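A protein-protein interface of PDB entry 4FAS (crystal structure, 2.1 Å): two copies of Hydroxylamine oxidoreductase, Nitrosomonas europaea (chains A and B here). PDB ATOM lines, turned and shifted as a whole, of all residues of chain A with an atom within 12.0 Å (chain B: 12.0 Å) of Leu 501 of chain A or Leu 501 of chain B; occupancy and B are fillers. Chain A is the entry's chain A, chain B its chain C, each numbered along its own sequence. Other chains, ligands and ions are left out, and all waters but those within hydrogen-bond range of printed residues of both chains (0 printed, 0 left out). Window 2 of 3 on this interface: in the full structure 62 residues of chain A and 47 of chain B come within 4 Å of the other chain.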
ATOM      1  N   SER A 492      -5.752  16.030  21.427  1.00  0.00           N
ATOM      2  CA  SER A 492      -4.590  16.696  20.919  1.00  0.00           C
ATOM      3  C   SER A 492      -4.146  17.800  21.897  1.00  0.00           C
ATOM      4  O   SER A 492      -2.960  18.100  22.003  1.00  0.00           O
ATOM      5  CB  SER A 492      -4.926  17.281  19.579  1.00  0.00           C
ATOM      6  OG  SER A 492      -3.962  18.231  19.268  1.00  0.00           O
ATOM      7  N   ALA A 493      -5.103  18.405  22.593  1.00  0.00           N
ATOM      8  CA  ALA A 493      -4.832  19.436  23.581  1.00  0.00           C
ATOM      9  C   ALA A 493      -4.242  18.787  24.824  1.00  0.00           C
ATOM     10  O   ALA A 493      -3.294  19.308  25.393  1.00  0.00           O
ATOM     11  CB  ALA A 493      -6.100  20.181  23.926  1.00  0.00           C
ATOM     12  N   LEU A 494      -4.780  17.632  25.215  1.00  0.00           N
ATOM     13  CA  LEU A 494      -4.287  16.897  26.357  1.00  0.00           C
ATOM     14  C   LEU A 494      -2.843  16.428  26.166  1.00  0.00           C
ATOM     15  O   LEU A 494      -2.074  16.367  27.115  1.00  0.00           O
ATOM     16  CB  LEU A 494      -5.182  15.695  26.645  1.00  0.00           C
ATOM     17  CG  LEU A 494      -4.762  14.994  27.943  1.00  0.00           C
ATOM     18  CD1 LEU A 494      -5.122  15.828  29.171  1.00  0.00           C
ATOM     19  CD2 LEU A 494      -5.286  13.575  28.048  1.00  0.00           C
ATOM     20  N   GLN A 495      -2.490  16.087  24.938  1.00  0.00           N
ATOM     21  CA  GLN A 495      -1.128  15.722  24.603  1.00  0.00           C
ATOM     22  C   GLN A 495      -0.160  16.881  24.593  1.00  0.00           C
ATOM     23  O   GLN A 495       0.970  16.749  25.073  1.00  0.00           O
ATOM     24  CB  GLN A 495      -1.080  15.048  23.249  1.00  0.00           C
ATOM     25  CG  GLN A 495      -1.107  13.593  23.403  1.00  0.00           C
ATOM     26  CD  GLN A 495      -0.674  12.882  22.178  1.00  0.00           C
ATOM     27  OE1 GLN A 495      -1.465  12.146  21.576  1.00  0.00           O
ATOM     28  NE2 GLN A 495       0.586  13.091  21.774  1.00  0.00           N
ATOM     29  N   ALA A 496      -0.602  18.004  24.021  1.00  0.00           N
ATOM     30  CA  ALA A 496       0.162  19.251  24.036  1.00  0.00           C
ATOM     31  C   ALA A 496       0.588  19.613  25.484  1.00  0.00           C
ATOM     32  O   ALA A 496       1.768  19.856  25.766  1.00  0.00           O
ATOM     33  CB  ALA A 496      -0.647  20.357  23.394  1.00  0.00           C
ATOM     34  N   ARG A 497      -0.382  19.598  26.389  1.00  0.00           N
ATOM     35  CA  ARG A 497      -0.161  19.729  27.820  1.00  0.00           C
ATOM     36  C   ARG A 497       0.896  18.789  28.412  1.00  0.00           C
ATOM     37  O   ARG A 497       1.620  19.195  29.306  1.00  0.00           O
ATOM     38  CB  ARG A 497      -1.465  19.463  28.557  1.00  0.00           C
ATOM     39  CG  ARG A 497      -2.577  20.404  28.249  1.00  0.00           C
ATOM     40  CD  ARG A 497      -3.177  20.881  29.546  1.00  0.00           C
ATOM     41  NE  ARG A 497      -4.630  20.756  29.577  1.00  0.00           N
ATOM     42  CZ  ARG A 497      -5.297  20.025  30.469  1.00  0.00           C
ATOM     43  NH1 ARG A 497      -4.642  19.357  31.426  1.00  0.00           N
ATOM     44  NH2 ARG A 497      -6.620  19.967  30.414  1.00  0.00           N
ATOM     45  N   VAL A 498       0.960  17.543  27.941  1.00  0.00           N
ATOM     46  CA  VAL A 498       1.911  16.532  28.451  1.00  0.00           C
ATOM     47  C   VAL A 498       3.369  16.663  27.894  1.00  0.00           C
ATOM     48  O   VAL A 498       4.339  16.339  28.599  1.00  0.00           O
ATOM     49  CB  VAL A 498       1.325  15.080  28.332  1.00  0.00           C
ATOM     50  CG1 VAL A 498       2.341  13.997  28.688  1.00  0.00           C
ATOM     51  CG2 VAL A 498       0.132  14.939  29.213  1.00  0.00           C
ATOM     52  N   ASN A 499       3.537  17.143  26.658  1.00  0.00           N
ATOM     53  CA  ASN A 499       4.869  17.577  26.208  1.00  0.00           C
ATOM     54  C   ASN A 499       5.286  18.682  27.118  1.00  0.00           C
ATOM     55  O   ASN A 499       6.223  18.521  27.880  1.00  0.00           O
ATOM     56  CB  ASN A 499       4.858  18.113  24.788  1.00  0.00           C
ATOM     57  CG  ASN A 499       4.291  17.140  23.833  1.00  0.00           C
ATOM     58  OD1 ASN A 499       4.277  15.937  24.098  1.00  0.00           O
ATOM     59  ND2 ASN A 499       3.790  17.637  22.715  1.00  0.00           N
ATOM     60  N   LYS A 500       4.552  19.792  27.046  1.00  0.00           N
ATOM     61  CA  LYS A 500       4.788  20.962  27.896  1.00  0.00           C
ATOM     62  C   LYS A 500       5.111  20.628  29.361  1.00  0.00           C
ATOM     63  O   LYS A 500       5.968  21.278  29.951  1.00  0.00           O
ATOM     64  CB  LYS A 500       3.639  21.985  27.788  1.00  0.00           C
ATOM     65  CG  LYS A 500       3.912  23.136  26.824  1.00  0.00           C
ATOM     66  CD  LYS A 500       4.854  24.173  27.456  1.00  0.00           C
ATOM     67  CE  LYS A 500       5.136  25.347  26.532  1.00  0.00           C
ATOM     68  NZ  LYS A 500       4.024  26.345  26.608  1.00  0.00           N
ATOM     69  N   LEU A 501       4.450  19.617  29.931  1.00  0.00           N
ATOM     70  CA  LEU A 501       4.791  19.137  31.275  1.00  0.00           C
ATOM     71  C   LEU A 501       6.154  18.472  31.383  1.00  0.00           C
ATOM     72  O   LEU A 501       6.765  18.520  32.424  1.00  0.00           O
ATOM     73  CB  LEU A 501       3.724  18.216  31.852  1.00  0.00           C
ATOM     74  CG  LEU A 501       2.959  18.856  33.009  1.00  0.00           C
ATOM     75  CD1 LEU A 501       2.213  20.078  32.513  1.00  0.00           C
ATOM     76  CD2 LEU A 501       2.001  17.866  33.651  1.00  0.00           C
ATOM     77  N   GLU A 502       6.632  17.859  30.312  1.00  0.00           N
ATOM     78  CA  GLU A 502       7.963  17.272  30.305  1.00  0.00           C
ATOM     79  C   GLU A 502       8.972  18.324  29.897  1.00  0.00           C
ATOM     80  O   GLU A 502       9.817  18.694  30.701  1.00  0.00           O
ATOM     81  CB  GLU A 502       8.032  16.122  29.320  1.00  0.00           C
ATOM     82  CG  GLU A 502       6.826  15.188  29.381  1.00  0.00           C
ATOM     83  CD  GLU A 502       6.778  14.225  28.198  1.00  0.00           C
ATOM     84  OE1 GLU A 502       6.436  13.040  28.418  1.00  0.00           O
ATOM     85  OE2 GLU A 502       7.084  14.654  27.049  1.00  0.00           O
ATOM     86  N   SER B 492      -2.830   4.590  25.232  1.00  0.00           N
ATOM     87  CA  SER B 492      -2.007   3.775  26.129  1.00  0.00           C
ATOM     88  C   SER B 492      -0.630   4.417  26.307  1.00  0.00           C
ATOM     89  O   SER B 492      -0.146   4.607  27.435  1.00  0.00           O
ATOM     90  CB  SER B 492      -1.837   2.405  25.522  1.00  0.00           C
ATOM     91  OG  SER B 492      -1.494   1.435  26.470  1.00  0.00           O
ATOM     92  N   ALA B 493      -0.013   4.750  25.176  1.00  0.00           N
ATOM     93  CA  ALA B 493       1.254   5.457  25.126  1.00  0.00           C
ATOM     94  C   ALA B 493       1.218   6.696  26.019  1.00  0.00           C
ATOM     95  O   ALA B 493       2.161   6.944  26.754  1.00  0.00           O
ATOM     96  CB  ALA B 493       1.581   5.859  23.699  1.00  0.00           C
ATOM     97  N   LEU B 494       0.118   7.446  25.955  1.00  0.00           N
ATOM     98  CA  LEU B 494       0.009   8.774  26.549  1.00  0.00           C
ATOM     99  C   LEU B 494      -0.237   8.611  28.013  1.00  0.00           C
ATOM    100  O   LEU B 494       0.260   9.386  28.801  1.00  0.00           O
ATOM    101  CB  LEU B 494      -1.103   9.597  25.899  1.00  0.00           C
ATOM    102  CG  LEU B 494      -1.306  10.994  26.500  1.00  0.00           C
ATOM    103  CD1 LEU B 494      -0.267  11.941  25.976  1.00  0.00           C
ATOM    104  CD2 LEU B 494      -2.687  11.530  26.206  1.00  0.00           C
ATOM    105  N   GLN B 495      -0.998   7.588  28.363  1.00  0.00           N
ATOM    106  CA  GLN B 495      -1.175   7.181  29.741  1.00  0.00           C
ATOM    107  C   GLN B 495       0.159   6.779  30.352  1.00  0.00           C
ATOM    108  O   GLN B 495       0.475   7.195  31.469  1.00  0.00           O
ATOM    109  CB  GLN B 495      -2.126   6.005  29.837  1.00  0.00           C
ATOM    110  CG  GLN B 495      -2.837   5.887  31.165  1.00  0.00           C
ATOM    111  CD  GLN B 495      -4.030   4.947  31.065  1.00  0.00           C
ATOM    112  OE1 GLN B 495      -4.330   4.225  32.015  1.00  0.00           O
ATOM    113  NE2 GLN B 495      -4.709   4.938  29.897  1.00  0.00           N
ATOM    114  N   ALA B 496       0.929   5.966  29.632  1.00  0.00           N
ATOM    115  CA  ALA B 496       2.281   5.616  30.065  1.00  0.00           C
ATOM    116  C   ALA B 496       3.109   6.886  30.405  1.00  0.00           C
ATOM    117  O   ALA B 496       3.674   6.998  31.508  1.00  0.00           O
ATOM    118  CB  ALA B 496       2.978   4.736  29.021  1.00  0.00           C
ATOM    119  N   ARG B 497       3.142   7.856  29.491  1.00  0.00           N
ATOM    120  CA  ARG B 497       3.843   9.122  29.733  1.00  0.00           C
ATOM    121  C   ARG B 497       3.407   9.821  31.010  1.00  0.00           C
ATOM    122  O   ARG B 497       4.174  10.559  31.621  1.00  0.00           O
ATOM    123  CB  ARG B 497       3.646  10.077  28.575  1.00  0.00           C
ATOM    124  CG  ARG B 497       4.015   9.476  27.272  1.00  0.00           C
ATOM    125  CD  ARG B 497       4.799  10.437  26.476  1.00  0.00           C
ATOM    126  NE  ARG B 497       4.010  11.233  25.539  1.00  0.00           N
ATOM    127  CZ  ARG B 497       4.043  12.559  25.493  1.00  0.00           C
ATOM    128  NH1 ARG B 497       4.807  13.226  26.339  1.00  0.00           N
ATOM    129  NH2 ARG B 497       3.329  13.226  24.601  1.00  0.00           N
ATOM    130  N   VAL B 498       2.178   9.584  31.418  1.00  0.00           N
ATOM    131  CA  VAL B 498       1.665  10.307  32.535  1.00  0.00           C
ATOM    132  C   VAL B 498       2.049   9.665  33.865  1.00  0.00           C
ATOM    133  O   VAL B 498       2.518  10.367  34.757  1.00  0.00           O
ATOM    134  CB  VAL B 498       0.173  10.673  32.352  1.00  0.00           C
ATOM    135  CG1 VAL B 498      -0.496  11.010  33.683  1.00  0.00           C
ATOM    136  CG2 VAL B 498       0.063  11.852  31.392  1.00  0.00           C
ATOM    137  N   ASN B 499       1.913   8.359  34.022  1.00  0.00           N
ATOM    138  CA  ASN B 499       2.411   7.808  35.279  1.00  0.00           C
ATOM    139  C   ASN B 499       3.968   7.771  35.383  1.00  0.00           C
ATOM    140  O   ASN B 499       4.537   7.574  36.481  1.00  0.00           O
ATOM    141  CB  ASN B 499       1.689   6.523  35.732  1.00  0.00           C
ATOM    142  CG  ASN B 499       1.779   5.401  34.734  1.00  0.00           C
ATOM    143  OD1 ASN B 499       0.810   4.686  34.494  1.00  0.00           O
ATOM    144  ND2 ASN B 499       2.947   5.214  34.169  1.00  0.00           N
ATOM    145  N   LYS B 500       4.645   8.021  34.255  1.00  0.00           N
ATOM    146  CA  LYS B 500       6.083   8.360  34.273  1.00  0.00           C
ATOM    147  C   LYS B 500       6.283   9.677  35.038  1.00  0.00           C
ATOM    148  O   LYS B 500       6.907   9.686  36.088  1.00  0.00           O
ATOM    149  CB  LYS B 500       6.635   8.457  32.859  1.00  0.00           C
ATOM    150  CG  LYS B 500       8.141   8.355  32.745  1.00  0.00           C
ATOM    151  CD  LYS B 500       8.609   9.015  31.452  1.00  0.00           C
ATOM    152  CE  LYS B 500       8.317  10.524  31.477  1.00  0.00           C
ATOM    153  NZ  LYS B 500       7.539  10.996  30.282  1.00  0.00           N
ATOM    154  N   LEU B 501       5.707  10.766  34.525  1.00  0.00           N
ATOM    155  CA  LEU B 501       5.673  12.057  35.217  1.00  0.00           C
ATOM    156  C   LEU B 501       5.239  11.971  36.681  1.00  0.00           C
ATOM    157  O   LEU B 501       5.616  12.806  37.486  1.00  0.00           O
ATOM    158  CB  LEU B 501       4.784  13.046  34.463  1.00  0.00           C
ATOM    159  CG  LEU B 501       5.508  13.947  33.466  1.00  0.00           C
ATOM    160  CD1 LEU B 501       6.573  13.218  32.683  1.00  0.00           C
ATOM    161  CD2 LEU B 501       4.536  14.585  32.523  1.00  0.00           C
ATOM    162  N   GLU B 502       4.443  10.964  37.018  1.00  0.00           N
ATOM    163  CA  GLU B 502       4.197  10.616  38.404  1.00  0.00           C
ATOM    164  C   GLU B 502       5.145   9.472  38.701  1.00  0.00           C
ATOM    165  O   GLU B 502       5.692   9.412  39.780  1.00  0.00           O
ATOM    166  CB  GLU B 502       2.755  10.152  38.627  1.00  0.00           C
ATOM    167  CG  GLU B 502       1.684  11.045  37.990  1.00  0.00           C
ATOM    168  CD  GLU B 502       0.315  10.361  37.839  1.00  0.00           C
ATOM    169  OE1 GLU B 502       0.245   9.111  37.817  1.00  0.00           O
ATOM    170  OE2 GLU B 502      -0.698  11.086  37.725  1.00  0.00           O
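Hydrophobic or aromatic side chains of chain B within 4 Å of the printed part of chain A: Leu 494, Val 498 and Leu 501.
Of the 11 printed residues of chain A, 6 touch a printed residue of chain B.
Hydrophobic or aromatic side chains of chain A within 4 Å of the printed part of chain B: Leu 494, Val 498 and Leu 501.
Among the printed residues, 10 pairs touch across the chains.
Among the printed residues, Asp or Glu carboxylates within 4 Å of a Lys or Arg side-chain nitrogen of the other chain: Glu 502 of chain A with Arg 497 of chain B (2.6 Å) and Glu 502 of chain A with Lys 500 of chain B (3.0 Å).
Of the printed residues of chain B, Gln 495 of chain A touches Leu 494 (3.2 Å) and Arg 497 (3.9 Å).
Of chain B, only Arg 497 (3.5 Å) and Val 498 (3.8 Å) come within 4 Å of Val 498 of chain A.
No residue of chain B comes within 4 Å of Lys 500 of chain A.
Leu 501 of chain A touches just one residue of chain B: Leu 501.
Glu 502 of chain A touches just these residues of chain B: Arg 497, Lys 500 and Leu 501.
Of the printed residues of chain A, Leu 494 of chain B touches Leu 494 and Gln 495.
Ala 496 of chain B touches none of the printed residues of chain A.
Printed residues of chain A within 4 Å of Arg 497 of chain B: Gln 495 (3.9 Å), Val 498 (3.5 Å), Asn 499 (2.9 Å) and Glu 502 (2.6 Å).
No residue of chain A comes within 4 Å of Asn 499 of chain B.
Lys 500 of chain B touches one residue of chain A.
Of chain A, only Leu 501 and Glu 502 come within 4 Å of Leu 501 of chain B.
No residue of chain A comes within 4 Å of Glu 502 of chain B.
The nearest residue of chain B that does not touch Leu 501 of chain A is Val 498 of chain B (6.7 Å).
The nearest printed residue of chain A that does not touch Leu 494 of chain B is Val 498 of chain A (4.2 Å).
OD1 of Asn 499 of chain A lies within hydrogen-bond range of NH2 of Arg 497 of chain B.
The guanidinium group (NH1) of Arg 497 of chain B lies within salt-bridge range of the side-chain carboxylate (OE1) of Glu 502 of chain A (2.6 Å).
OE1 of Glu 502 of chain A is in salt-bridge range of NZ of Lys 500 of chain B, 3.0 Å away.
Val 498 of chain A touches Arg 497 of chain B, but with the chains exchanged Arg 497 of chain A does not touch Val 498 of chain B (7.6 Å).
Val 498 of chain B touches its own counterpart, Val 498 of chain A.
Glu 502 of chain A touches Arg 497 of chain B, but with the chains exchanged Arg 497 of chain A does not touch Glu 502 of chain B (11.1 Å).
Glu 502 of chain A touches Leu 501 of chain B, but with the chains exchanged Leu 501 of chain A does not touch Glu 502 of chain B (8.1 Å).
Of the 10 pairs that touch across the chains among the printed residues, 3 have their exchanged pair printed and touching as well.
Leu 494 of chain B touches Leu 494 of chain A.
Leu 494 of chain B touches Gln 495 of chain A.
Arg 497 of chain B touches Gln 495 of chain A (NH2 to NE2, 3.9 Å).
CG1 of Val 498 of chain A touches NH1 of Arg 497 of chain B, 3.5 Å away.
Val 498 of chain A touches Val 498 of chain B.
Leu 501 of chain A touches Leu 501 of chain B.
Glu 502 of chain A touches Leu 501 of chain B (CG to CD1, 3.9 Å).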
